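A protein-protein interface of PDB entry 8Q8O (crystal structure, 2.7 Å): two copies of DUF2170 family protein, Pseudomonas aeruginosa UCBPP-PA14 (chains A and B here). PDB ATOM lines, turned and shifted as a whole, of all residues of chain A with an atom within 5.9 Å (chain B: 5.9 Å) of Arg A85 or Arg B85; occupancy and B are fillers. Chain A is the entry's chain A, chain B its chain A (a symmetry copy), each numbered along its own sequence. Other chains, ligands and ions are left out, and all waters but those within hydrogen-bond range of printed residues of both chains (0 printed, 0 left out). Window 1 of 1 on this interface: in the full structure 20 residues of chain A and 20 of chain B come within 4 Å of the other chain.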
ATOM      1  N   GLN A  58      -5.561   8.754  -2.000  1.00  0.00           N
ATOM      2  CA  GLN A  58      -6.342   9.972  -2.166  1.00  0.00           C
ATOM      3  C   GLN A  58      -7.352   9.765  -3.287  1.00  0.00           C
ATOM      4  O   GLN A  58      -7.160   8.927  -4.172  1.00  0.00           O
ATOM      5  CB  GLN A  58      -5.448  11.177  -2.480  1.00  0.00           C
ATOM      6  CG  GLN A  58      -4.583  10.995  -3.720  1.00  0.00           C
ATOM      7  CD  GLN A  58      -3.754  12.225  -4.050  1.00  0.00           C
ATOM      8  OE1 GLN A  58      -3.855  13.257  -3.384  1.00  0.00           O
ATOM      9  NE2 GLN A  58      -2.931  12.122  -5.088  1.00  0.00           N
ATOM     10  N   GLU A  80       3.913  32.633 -10.505  1.00  0.00           N
ATOM     11  CA  GLU A  80       2.711  33.217  -9.918  1.00  0.00           C
ATOM     12  C   GLU A  80       1.786  32.137  -9.374  1.00  0.00           C
ATOM     13  O   GLU A  80       1.140  32.326  -8.335  1.00  0.00           O
ATOM     14  CB  GLU A  80       1.986  34.080 -10.951  1.00  0.00           C
ATOM     15  CG  GLU A  80       0.653  34.640 -10.468  1.00  0.00           C
ATOM     16  CD  GLU A  80       0.792  35.499  -9.222  1.00  0.00           C
ATOM     17  OE1 GLU A  80       1.830  36.180  -9.077  1.00  0.00           O
ATOM     18  OE2 GLU A  80      -0.140  35.489  -8.386  1.00  0.00           O
ATOM     19  N   VAL A  81       1.708  30.995 -10.062  1.00  0.00           N
ATOM     20  CA  VAL A  81       0.872  29.897  -9.586  1.00  0.00           C
ATOM     21  C   VAL A  81       1.323  29.444  -8.204  1.00  0.00           C
ATOM     22  O   VAL A  81       0.500  29.212  -7.310  1.00  0.00           O
ATOM     23  CB  VAL A  81       0.891  28.734 -10.594  1.00  0.00           C
ATOM     24  CG1 VAL A  81       0.392  27.459  -9.935  1.00  0.00           C
ATOM     25  CG2 VAL A  81       0.050  29.076 -11.809  1.00  0.00           C
ATOM     26  N   LEU A  82       2.636  29.309  -8.006  1.00  0.00           N
ATOM     27  CA  LEU A  82       3.159  28.870  -6.717  1.00  0.00           C
ATOM     28  C   LEU A  82       3.016  29.937  -5.641  1.00  0.00           C
ATOM     29  O   LEU A  82       2.950  29.597  -4.455  1.00  0.00           O
ATOM     30  CB  LEU A  82       4.626  28.463  -6.861  1.00  0.00           C
ATOM     31  CG  LEU A  82       4.929  27.392  -7.910  1.00  0.00           C
ATOM     32  CD1 LEU A  82       6.420  27.109  -7.975  1.00  0.00           C
ATOM     33  CD2 LEU A  82       4.158  26.122  -7.614  1.00  0.00           C
ATOM     34  N   LEU A  83       2.965  31.214  -6.026  1.00  0.00           N
ATOM     35  CA  LEU A  83       2.823  32.293  -5.057  1.00  0.00           C
ATOM     36  C   LEU A  83       1.382  32.511  -4.619  1.00  0.00           C
ATOM     37  O   LEU A  83       1.157  33.135  -3.577  1.00  0.00           O
ATOM     38  CB  LEU A  83       3.375  33.599  -5.638  1.00  0.00           C
ATOM     39  CG  LEU A  83       4.893  33.736  -5.764  1.00  0.00           C
ATOM     40  CD1 LEU A  83       5.243  34.920  -6.649  1.00  0.00           C
ATOM     41  CD2 LEU A  83       5.541  33.877  -4.395  1.00  0.00           C
ATOM     42  N   SER A  84       0.405  32.015  -5.373  1.00  0.00           N
ATOM     43  CA  SER A  84      -1.002  32.315  -5.138  1.00  0.00           C
ATOM     44  C   SER A  84      -1.819  31.053  -4.873  1.00  0.00           C
ATOM     45  O   SER A  84      -2.945  30.908  -5.353  1.00  0.00           O
ATOM     46  CB  SER A  84      -1.586  33.102  -6.311  1.00  0.00           C
ATOM     47  OG  SER A  84      -1.285  32.481  -7.550  1.00  0.00           O
ATOM     48  N   ARG A  85      -1.262  30.125  -4.091  1.00  0.00           N
ATOM     49  CA  ARG A  85      -2.041  28.974  -3.643  1.00  0.00           C
ATOM     50  C   ARG A  85      -3.313  29.416  -2.935  1.00  0.00           C
ATOM     51  O   ARG A  85      -4.371  28.797  -3.091  1.00  0.00           O
ATOM     52  CB  ARG A  85      -1.203  28.103  -2.711  1.00  0.00           C
ATOM     53  CG  ARG A  85       0.098  27.644  -3.312  1.00  0.00           C
ATOM     54  CD  ARG A  85      -0.142  27.054  -4.679  1.00  0.00           C
ATOM     55  NE  ARG A  85       0.913  26.120  -5.043  1.00  0.00           N
ATOM     56  CZ  ARG A  85       0.898  25.375  -6.140  1.00  0.00           C
ATOM     57  NH1 ARG A  85      -0.122  25.457  -6.983  1.00  0.00           N
ATOM     58  NH2 ARG A  85       1.903  24.549  -6.387  1.00  0.00           N
ATOM     59  N   GLN A  86      -3.224  30.488  -2.144  1.00  0.00           N
ATOM     60  CA  GLN A  86      -4.370  30.953  -1.372  1.00  0.00           C
ATOM     61  C   GLN A  86      -5.564  31.270  -2.264  1.00  0.00           C
ATOM     62  O   GLN A  86      -6.710  31.222  -1.802  1.00  0.00           O
ATOM     63  CB  GLN A  86      -3.973  32.185  -0.557  1.00  0.00           C
ATOM     64  CG  GLN A  86      -3.575  33.384  -1.414  1.00  0.00           C
ATOM     65  CD  GLN A  86      -2.073  33.481  -1.641  1.00  0.00           C
ATOM     66  OE1 GLN A  86      -1.345  32.497  -1.491  1.00  0.00           O
ATOM     67  NE2 GLN A  86      -1.604  34.672  -2.007  1.00  0.00           N
ATOM     68  N   LEU A  87      -5.322  31.584  -3.539  1.00  0.00           N
ATOM     69  CA  LEU A  87      -6.401  32.043  -4.410  1.00  0.00           C
ATOM     70  C   LEU A  87      -7.539  31.032  -4.476  1.00  0.00           C
ATOM     71  O   LEU A  87      -8.716  31.412  -4.480  1.00  0.00           O
ATOM     72  CB  LEU A  87      -5.860  32.327  -5.811  1.00  0.00           C
ATOM     73  CG  LEU A  87      -5.237  33.705  -6.047  1.00  0.00           C
ATOM     74  CD1 LEU A  87      -4.733  33.817  -7.476  1.00  0.00           C
ATOM     75  CD2 LEU A  87      -6.231  34.814  -5.732  1.00  0.00           C
ATOM     76  N   PHE A  88      -7.213  29.747  -4.532  1.00  0.00           N
ATOM     77  CA  PHE A  88      -8.215  28.704  -4.743  1.00  0.00           C
ATOM     78  C   PHE A  88      -8.222  27.733  -3.575  1.00  0.00           C
ATOM     79  O   PHE A  88      -7.264  26.953  -3.415  1.00  0.00           O
ATOM     80  CB  PHE A  88      -7.943  27.973  -6.056  1.00  0.00           C
ATOM     81  CG  PHE A  88      -7.510  28.881  -7.165  1.00  0.00           C
ATOM     82  CD1 PHE A  88      -8.441  29.629  -7.868  1.00  0.00           C
ATOM     83  CD2 PHE A  88      -6.169  29.007  -7.490  1.00  0.00           C
ATOM     84  CE1 PHE A  88      -8.043  30.475  -8.884  1.00  0.00           C
ATOM     85  CE2 PHE A  88      -5.765  29.851  -8.506  1.00  0.00           C
ATOM     86  CZ  PHE A  88      -6.704  30.588  -9.204  1.00  0.00           C
ATOM     87  N   PRO A  89      -9.258  27.739  -2.739  1.00  0.00           N
ATOM     88  CA  PRO A  89      -9.309  26.796  -1.619  1.00  0.00           C
ATOM     89  C   PRO A  89      -9.654  25.389  -2.083  1.00  0.00           C
ATOM     90  O   PRO A  89     -10.514  25.186  -2.944  1.00  0.00           O
ATOM     91  CB  PRO A  89     -10.415  27.371  -0.727  1.00  0.00           C
ATOM     92  CG  PRO A  89     -11.316  28.084  -1.686  1.00  0.00           C
ATOM     93  CD  PRO A  89     -10.421  28.643  -2.761  1.00  0.00           C
ATOM     94  N   SER A  91      -8.120  23.261  -3.866  1.00  0.00           N
ATOM     95  CA  SER A  91      -7.579  22.780  -5.128  1.00  0.00           C
ATOM     96  C   SER A  91      -6.321  23.562  -5.480  1.00  0.00           C
ATOM     97  O   SER A  91      -6.096  24.672  -4.991  1.00  0.00           O
ATOM     98  CB  SER A  91      -8.606  22.890  -6.265  1.00  0.00           C
ATOM     99  OG  SER A  91      -9.190  24.181  -6.304  1.00  0.00           O
ATOM    100  N   SER A  92      -5.499  22.963  -6.339  1.00  0.00           N
ATOM    101  CA  SER A  92      -4.251  23.570  -6.779  1.00  0.00           C
ATOM    102  C   SER A  92      -4.058  23.304  -8.264  1.00  0.00           C
ATOM    103  O   SER A  92      -4.604  22.349  -8.823  1.00  0.00           O
ATOM    104  CB  SER A  92      -3.055  23.043  -5.974  1.00  0.00           C
ATOM    105  OG  SER A  92      -3.134  21.639  -5.804  1.00  0.00           O
ATOM    106  N   ILE A  93      -3.265  24.163  -8.901  1.00  0.00           N
ATOM    107  CA  ILE A  93      -3.063  24.131 -10.346  1.00  0.00           C
ATOM    108  C   ILE A  93      -1.889  23.220 -10.678  1.00  0.00           C
ATOM    109  O   ILE A  93      -0.898  23.157  -9.945  1.00  0.00           O
ATOM    110  CB  ILE A  93      -2.841  25.555 -10.894  1.00  0.00           C
ATOM    111  CG1 ILE A  93      -4.058  26.435 -10.598  1.00  0.00           C
ATOM    112  CG2 ILE A  93      -2.551  25.514 -12.387  1.00  0.00           C
ATOM    113  CD1 ILE A  93      -3.946  27.841 -11.149  1.00  0.00           C
ATOM    114  N   GLY A  94      -1.994  22.510 -11.806  1.00  0.00           N
ATOM    115  CA  GLY A  94      -0.951  21.606 -12.241  1.00  0.00           C
ATOM    116  C   GLY A  94      -0.739  21.676 -13.744  1.00  0.00           C
ATOM    117  O   GLY A  94      -1.411  22.429 -14.450  1.00  0.00           O
ATOM    118  N   LEU A  95       0.218  20.876 -14.212  1.00  0.00           N
ATOM    119  CA  LEU A  95       0.545  20.752 -15.628  1.00  0.00           C
ATOM    120  C   LEU A  95       0.429  19.291 -16.040  1.00  0.00           C
ATOM    121  O   LEU A  95       0.967  18.409 -15.362  1.00  0.00           O
ATOM    122  CB  LEU A  95       1.960  21.261 -15.915  1.00  0.00           C
ATOM    123  CG  LEU A  95       2.127  22.607 -16.621  1.00  0.00           C
ATOM    124  CD1 LEU A  95       3.585  22.810 -16.995  1.00  0.00           C
ATOM    125  CD2 LEU A  95       1.236  22.701 -17.851  1.00  0.00           C
ATOM    126  N   PHE A 108      -6.643  20.561  -9.827  1.00  0.00           N
ATOM    127  CA  PHE A 108      -6.903  19.292  -9.167  1.00  0.00           C
ATOM    128  C   PHE A 108      -7.120  19.496  -7.675  1.00  0.00           C
ATOM    129  O   PHE A 108      -6.495  20.362  -7.054  1.00  0.00           O
ATOM    130  CB  PHE A 108      -5.754  18.303  -9.400  1.00  0.00           C
ATOM    131  CG  PHE A 108      -4.587  18.502  -8.481  1.00  0.00           C
ATOM    132  CD1 PHE A 108      -3.585  19.403  -8.800  1.00  0.00           C
ATOM    133  CD2 PHE A 108      -4.483  17.780  -7.301  1.00  0.00           C
ATOM    134  CE1 PHE A 108      -2.503  19.586  -7.958  1.00  0.00           C
ATOM    135  CE2 PHE A 108      -3.403  17.960  -6.452  1.00  0.00           C
ATOM    136  CZ  PHE A 108      -2.412  18.863  -6.782  1.00  0.00           C
ATOM    137  N   TYR A 138      -6.644  35.170 -13.514  1.00  0.00           N
ATOM    138  CA  TYR A 138      -5.397  35.002 -14.249  1.00  0.00           C
ATOM    139  C   TYR A 138      -5.494  35.482 -15.691  1.00  0.00           C
ATOM    140  O   TYR A 138      -4.554  35.274 -16.465  1.00  0.00           O
ATOM    141  CB  TYR A 138      -4.960  33.537 -14.221  1.00  0.00           C
ATOM    142  CG  TYR A 138      -4.391  33.076 -12.900  1.00  0.00           C
ATOM    143  CD1 TYR A 138      -3.632  33.929 -12.111  1.00  0.00           C
ATOM    144  CD2 TYR A 138      -4.617  31.785 -12.439  1.00  0.00           C
ATOM    145  CE1 TYR A 138      -3.110  33.506 -10.900  1.00  0.00           C
ATOM    146  CE2 TYR A 138      -4.100  31.354 -11.234  1.00  0.00           C
ATOM    147  CZ  TYR A 138      -3.348  32.217 -10.467  1.00  0.00           C
ATOM    148  OH  TYR A 138      -2.836  31.785  -9.265  1.00  0.00           O
ATOM    149  N   GLN B  58     -11.506  26.367   4.252  1.00  0.00           N
ATOM    150  CA  GLN B  58     -10.586  25.239   4.298  1.00  0.00           C
ATOM    151  C   GLN B  58      -9.732  25.345   5.554  1.00  0.00           C
ATOM    152  O   GLN B  58      -9.538  26.433   6.103  1.00  0.00           O
ATOM    153  CB  GLN B  58      -9.690  25.190   3.056  1.00  0.00           C
ATOM    154  CG  GLN B  58      -8.876  26.458   2.835  1.00  0.00           C
ATOM    155  CD  GLN B  58      -7.946  26.364   1.636  1.00  0.00           C
ATOM    156  OE1 GLN B  58      -7.858  25.324   0.981  1.00  0.00           O
ATOM    157  NE2 GLN B  58      -7.243  27.453   1.347  1.00  0.00           N
ATOM    158  N   GLU B  80       8.741  21.692 -13.083  1.00  0.00           N
ATOM    159  CA  GLU B  80       8.715  20.314 -12.603  1.00  0.00           C
ATOM    160  C   GLU B  80       7.711  20.148 -11.470  1.00  0.00           C
ATOM    161  O   GLU B  80       7.043  19.111 -11.367  1.00  0.00           O
ATOM    162  CB  GLU B  80      10.112  19.886 -12.153  1.00  0.00           C
ATOM    163  CG  GLU B  80      10.165  18.499 -11.524  1.00  0.00           C
ATOM    164  CD  GLU B  80       9.667  17.408 -12.458  1.00  0.00           C
ATOM    165  OE1 GLU B  80       9.874  17.531 -13.685  1.00  0.00           O
ATOM    166  OE2 GLU B  80       9.067  16.429 -11.962  1.00  0.00           O
ATOM    167  N   VAL B  81       7.589  21.160 -10.607  1.00  0.00           N
ATOM    168  CA  VAL B  81       6.621  21.093  -9.516  1.00  0.00           C
ATOM    169  C   VAL B  81       5.211  20.926 -10.062  1.00  0.00           C
ATOM    170  O   VAL B  81       4.423  20.117  -9.556  1.00  0.00           O
ATOM    171  CB  VAL B  81       6.735  22.342  -8.623  1.00  0.00           C
ATOM    172  CG1 VAL B  81       5.489  22.490  -7.765  1.00  0.00           C
ATOM    173  CG2 VAL B  81       7.978  22.259  -7.757  1.00  0.00           C
ATOM    174  N   LEU B  82       4.867  21.688 -11.104  1.00  0.00           N
ATOM    175  CA  LEU B  82       3.534  21.603 -11.687  1.00  0.00           C
ATOM    176  C   LEU B  82       3.318  20.305 -12.452  1.00  0.00           C
ATOM    177  O   LEU B  82       2.172  19.861 -12.584  1.00  0.00           O
ATOM    178  CB  LEU B  82       3.288  22.799 -12.608  1.00  0.00           C
ATOM    179  CG  LEU B  82       3.467  24.181 -11.977  1.00  0.00           C
ATOM    180  CD1 LEU B  82       3.232  25.276 -13.003  1.00  0.00           C
ATOM    181  CD2 LEU B  82       2.537  24.352 -10.793  1.00  0.00           C
ATOM    182  N   LEU B  83       4.390  19.687 -12.954  1.00  0.00           N
ATOM    183  CA  LEU B  83       4.267  18.437 -13.694  1.00  0.00           C
ATOM    184  C   LEU B  83       4.161  17.220 -12.787  1.00  0.00           C
ATOM    185  O   LEU B  83       3.716  16.163 -13.247  1.00  0.00           O
ATOM    186  CB  LEU B  83       5.464  18.261 -14.633  1.00  0.00           C
ATOM    187  CG  LEU B  83       5.525  19.144 -15.880  1.00  0.00           C
ATOM    188  CD1 LEU B  83       6.910  19.082 -16.503  1.00  0.00           C
ATOM    189  CD2 LEU B  83       4.462  18.734 -16.889  1.00  0.00           C
ATOM    190  N   SER B  84       4.548  17.334 -11.519  1.00  0.00           N
ATOM    191  CA  SER B  84       4.650  16.191 -10.619  1.00  0.00           C
ATOM    192  C   SER B  84       3.752  16.345  -9.396  1.00  0.00           C
ATOM    193  O   SER B  84       4.141  16.014  -8.273  1.00  0.00           O
ATOM    194  CB  SER B  84       6.103  15.965 -10.202  1.00  0.00           C
ATOM    195  OG  SER B  84       6.701  17.167  -9.746  1.00  0.00           O
ATOM    196  N   ARG B  85       2.531  16.843  -9.599  1.00  0.00           N
ATOM    197  CA  ARG B  85       1.551  16.858  -8.517  1.00  0.00           C
ATOM    198  C   ARG B  85       1.349  15.463  -7.944  1.00  0.00           C
ATOM    199  O   ARG B  85       1.189  15.297  -6.729  1.00  0.00           O
ATOM    200  CB  ARG B  85       0.220  17.411  -9.021  1.00  0.00           C
ATOM    201  CG  ARG B  85       0.324  18.778  -9.642  1.00  0.00           C
ATOM    202  CD  ARG B  85       1.086  19.704  -8.728  1.00  0.00           C
ATOM    203  NE  ARG B  85       0.737  21.095  -8.979  1.00  0.00           N
ATOM    204  CZ  ARG B  85       1.174  22.112  -8.247  1.00  0.00           C
ATOM    205  NH1 ARG B  85       1.979  21.891  -7.217  1.00  0.00           N
ATOM    206  NH2 ARG B  85       0.800  23.347  -8.549  1.00  0.00           N
ATOM    207  N   GLN B  86       1.345  14.447  -8.810  1.00  0.00           N
ATOM    208  CA  GLN B  86       1.096  13.080  -8.368  1.00  0.00           C
ATOM    209  C   GLN B  86       2.093  12.636  -7.305  1.00  0.00           C
ATOM    210  O   GLN B  86       1.787  11.746  -6.504  1.00  0.00           O
ATOM    211  CB  GLN B  86       1.145  12.136  -9.570  1.00  0.00           C
ATOM    212  CG  GLN B  86       2.512  12.078 -10.247  1.00  0.00           C
ATOM    213  CD  GLN B  86       2.631  13.028 -11.430  1.00  0.00           C
ATOM    214  OE1 GLN B  86       1.868  13.990 -11.549  1.00  0.00           O
ATOM    215  NE2 GLN B  86       3.594  12.764 -12.310  1.00  0.00           N
ATOM    216  N   LEU B  87       3.281  13.246  -7.273  1.00  0.00           N
ATOM    217  CA  LEU B  87       4.337  12.772  -6.381  1.00  0.00           C
ATOM    218  C   LEU B  87       3.879  12.752  -4.928  1.00  0.00           C
ATOM    219  O   LEU B  87       4.201  11.820  -4.181  1.00  0.00           O
ATOM    220  CB  LEU B  87       5.582  13.642  -6.535  1.00  0.00           C
ATOM    221  CG  LEU B  87       6.541  13.287  -7.673  1.00  0.00           C
ATOM    222  CD1 LEU B  87       7.711  14.256  -7.700  1.00  0.00           C
ATOM    223  CD2 LEU B  87       7.029  11.850  -7.548  1.00  0.00           C
ATOM    224  N   PHE B  88       3.134  13.765  -4.507  1.00  0.00           N
ATOM    225  CA  PHE B  88       2.763  13.921  -3.102  1.00  0.00           C
ATOM    226  C   PHE B  88       1.251  13.912  -2.950  1.00  0.00           C
ATOM    227  O   PHE B  88       0.583  14.879  -3.362  1.00  0.00           O
ATOM    228  CB  PHE B  88       3.356  15.212  -2.542  1.00  0.00           C
ATOM    229  CG  PHE B  88       4.749  15.483  -3.020  1.00  0.00           C
ATOM    230  CD1 PHE B  88       5.830  14.834  -2.449  1.00  0.00           C
ATOM    231  CD2 PHE B  88       4.977  16.372  -4.060  1.00  0.00           C
ATOM    232  CE1 PHE B  88       7.115  15.074  -2.895  1.00  0.00           C
ATOM    233  CE2 PHE B  88       6.259  16.616  -4.511  1.00  0.00           C
ATOM    234  CZ  PHE B  88       7.331  15.967  -3.928  1.00  0.00           C
ATOM    235  N   PRO B  89       0.669  12.860  -2.380  1.00  0.00           N
ATOM    236  CA  PRO B  89      -0.784  12.831  -2.192  1.00  0.00           C
ATOM    237  C   PRO B  89      -1.222  13.732  -1.048  1.00  0.00           C
ATOM    238  O   PRO B  89      -0.585  13.791   0.007  1.00  0.00           O
ATOM    239  CB  PRO B  89      -1.067  11.359  -1.877  1.00  0.00           C
ATOM    240  CG  PRO B  89       0.196  10.879  -1.232  1.00  0.00           C
ATOM    241  CD  PRO B  89       1.317  11.623  -1.911  1.00  0.00           C
ATOM    242  N   SER B  91      -1.184  16.877  -0.632  1.00  0.00           N
ATOM    243  CA  SER B  91      -0.502  18.147  -0.432  1.00  0.00           C
ATOM    244  C   SER B  91       0.143  18.595  -1.736  1.00  0.00           C
ATOM    245  O   SER B  91       0.394  17.793  -2.638  1.00  0.00           O
ATOM    246  CB  SER B  91       0.555  18.055   0.678  1.00  0.00           C
ATOM    247  OG  SER B  91       1.399  16.935   0.490  1.00  0.00           O
ATOM    248  N   SER B  92       0.409  19.897  -1.822  1.00  0.00           N
ATOM    249  CA  SER B  92       1.022  20.491  -3.001  1.00  0.00           C
ATOM    250  C   SER B  92       2.037  21.540  -2.565  1.00  0.00           C
ATOM    251  O   SER B  92       1.960  22.091  -1.464  1.00  0.00           O
ATOM    252  CB  SER B  92      -0.030  21.112  -3.930  1.00  0.00           C
ATOM    253  OG  SER B  92      -0.994  21.842  -3.193  1.00  0.00           O
ATOM    254  N   ILE B  93       2.995  21.811  -3.450  1.00  0.00           N
ATOM    255  CA  ILE B  93       4.114  22.698  -3.155  1.00  0.00           C
ATOM    256  C   ILE B  93       3.745  24.127  -3.523  1.00  0.00           C
ATOM    257  O   ILE B  93       3.043  24.377  -4.505  1.00  0.00           O
ATOM    258  CB  ILE B  93       5.383  22.236  -3.902  1.00  0.00           C
ATOM    259  CG1 ILE B  93       5.765  20.818  -3.473  1.00  0.00           C
ATOM    260  CG2 ILE B  93       6.530  23.206  -3.658  1.00  0.00           C
ATOM    261  CD1 ILE B  93       7.034  20.303  -4.122  1.00  0.00           C
ATOM    262  N   GLY B  94       4.233  25.086  -2.728  1.00  0.00           N
ATOM    263  CA  GLY B  94       3.962  26.488  -2.963  1.00  0.00           C
ATOM    264  C   GLY B  94       5.189  27.348  -2.711  1.00  0.00           C
ATOM    265  O   GLY B  94       6.254  26.851  -2.348  1.00  0.00           O
ATOM    266  N   LEU B  95       5.011  28.652  -2.921  1.00  0.00           N
ATOM    267  CA  LEU B  95       6.045  29.655  -2.687  1.00  0.00           C
ATOM    268  C   LEU B  95       5.514  30.698  -1.714  1.00  0.00           C
ATOM    269  O   LEU B  95       4.404  31.211  -1.895  1.00  0.00           O
ATOM    270  CB  LEU B  95       6.464  30.330  -3.995  1.00  0.00           C
ATOM    271  CG  LEU B  95       7.815  29.965  -4.611  1.00  0.00           C
ATOM    272  CD1 LEU B  95       8.119  30.901  -5.767  1.00  0.00           C
ATOM    273  CD2 LEU B  95       8.926  30.014  -3.572  1.00  0.00           C
ATOM    274  N   PHE B 108       1.862  22.500   1.397  1.00  0.00           N
ATOM    275  CA  PHE B 108       0.601  22.785   2.060  1.00  0.00           C
ATOM    276  C   PHE B 108      -0.454  21.759   1.674  1.00  0.00           C
ATOM    277  O   PHE B 108      -0.486  21.275   0.536  1.00  0.00           O
ATOM    278  CB  PHE B 108       0.107  24.197   1.723  1.00  0.00           C
ATOM    279  CG  PHE B 108      -0.602  24.294   0.406  1.00  0.00           C
ATOM    280  CD1 PHE B 108       0.109  24.500  -0.764  1.00  0.00           C
ATOM    281  CD2 PHE B 108      -1.984  24.190   0.337  1.00  0.00           C
ATOM    282  CE1 PHE B 108      -0.542  24.595  -1.981  1.00  0.00           C
ATOM    283  CE2 PHE B 108      -2.643  24.283  -0.878  1.00  0.00           C
ATOM    284  CZ  PHE B 108      -1.921  24.486  -2.037  1.00  0.00           C
ATOM    285  N   TYR B 138      13.499  15.408  -5.032  1.00  0.00           N
ATOM    286  CA  TYR B 138      13.887  16.633  -5.719  1.00  0.00           C
ATOM    287  C   TYR B 138      15.334  17.025  -5.450  1.00  0.00           C
ATOM    288  O   TYR B 138      15.755  18.112  -5.859  1.00  0.00           O
ATOM    289  CB  TYR B 138      12.959  17.781  -5.321  1.00  0.00           C
ATOM    290  CG  TYR B 138      11.583  17.719  -5.939  1.00  0.00           C
ATOM    291  CD1 TYR B 138      11.398  17.237  -7.228  1.00  0.00           C
ATOM    292  CD2 TYR B 138      10.464  18.142  -5.232  1.00  0.00           C
ATOM    293  CE1 TYR B 138      10.136  17.183  -7.795  1.00  0.00           C
ATOM    294  CE2 TYR B 138       9.203  18.092  -5.789  1.00  0.00           C
ATOM    295  CZ  TYR B 138       9.042  17.610  -7.070  1.00  0.00           C
ATOM    296  OH  TYR B 138       7.784  17.561  -7.623  1.00  0.00           O
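O of Leu A83 lies close to OE1 of Gln A86 (3.3 Å).
O of Phe A108 is in hydrogen-bond range of N of Ser A92, 2.9 Å away.
The backbone carbonyl oxygen (O) of Leu B83 lies close to the side-chain amide oxygen (OE1) of Gln B86 (3.3 Å).
The backbone carbonyl oxygen of Phe B108 is in hydrogen-bond range of the backbone NH of Ser B92, at 2.9 Å.
Among the printed residues, pairs that only touch across the chains: Pro A89 with Gln B58 (3.3 Å), Gln A58 with Pro B89 (3.3 Å), Arg A85 with Phe B108 (3.4 Å), Phe A108 with Arg B85 (3.4 Å), Gly A94 with Leu B82 (3.6 Å), Leu A82 with Gly B94 (3.6 Å), Leu A83 with Leu B95 (3.7 Å), Leu A95 with Leu B83 (3.7 Å), Gly A94 with Arg B85 (3.7 Å), Arg A85 with Gly B94 (3.7 Å), Ile A93 with Leu B82 (3.7 Å), Leu A82 with Ile B93 (3.7 Å), Leu A82 with Val B81 (3.9 Å), Val A81 with Leu B82 (3.9 Å) and Leu A82 with Leu B82 (3.98 Å).
Hydrophobic or aromatic side chains of chain A within 4 Å of the printed part of chain B: Val A81, Leu A82, Leu A83, Pro A89, Leu A95 and Phe A108.
Among the printed residues, no Asp or Glu carboxylate lies within 4 Å of a Lys or Arg side-chain nitrogen of the other chain.
Leu A82 touches Ile B93, and with the chains exchanged Ile A93 touches Leu B82.
Leu A82 touches Leu B95, and with the chains exchanged Leu A95 touches Leu B82.
Leu A83 touches Leu B95, and with the chains exchanged Leu A95 touches Leu B83.
Arg A85 touches Gly B94, and with the chains exchanged Gly A94 touches Arg B85.
Of the 21 pairs that touch across the chains among the printed residues, 21 have their exchanged pair printed and touching as well.
Of the printed residues of chain A, Arg B85 touches Arg A85 (2.7 Å), Ile A93 (2.2 Å), Gly A94 (3.7 Å) and Phe A108 (3.4 Å).
Of the printed residues of chain A, Leu B82 touches Val A81 (3.9 Å), Leu A82 (3.98 Å), Ile A93 (3.7 Å), Gly A94 (3.6 Å) and Leu A95 (2.7 Å).
Printed residues of chain A within 4 Å of Leu B95: Leu A82 and Leu A83.
Phe A88 touches none of the printed residues of chain B.
The nearest printed residue of chain A that does not touch Phe B108 is Ser A92 (4.3 Å).
The backbone carbonyl oxygen (O) of Leu A82 is in hydrogen-bond range of the backbone NH (N) of Leu B95 (2.7 Å).
The guanidinium group (NH2) of Arg A85 lies close to the guanidinium group (NH2) of Arg B85, 2.7 Å away.
NE of Arg A85 sits at hydrogen-bond distance from O of Ile B93 (2.8 Å).
OG of Ser B92 sits at hydrogen-bond distance from OG of Ser A92 (3.4 Å).
The guanidinium group of Arg B85 sits at hydrogen-bond distance from the backbone carbonyl oxygen of Ile A93, 2.8 Å away.
N of Leu A95 lies within hydrogen-bond range of O of Leu B82.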
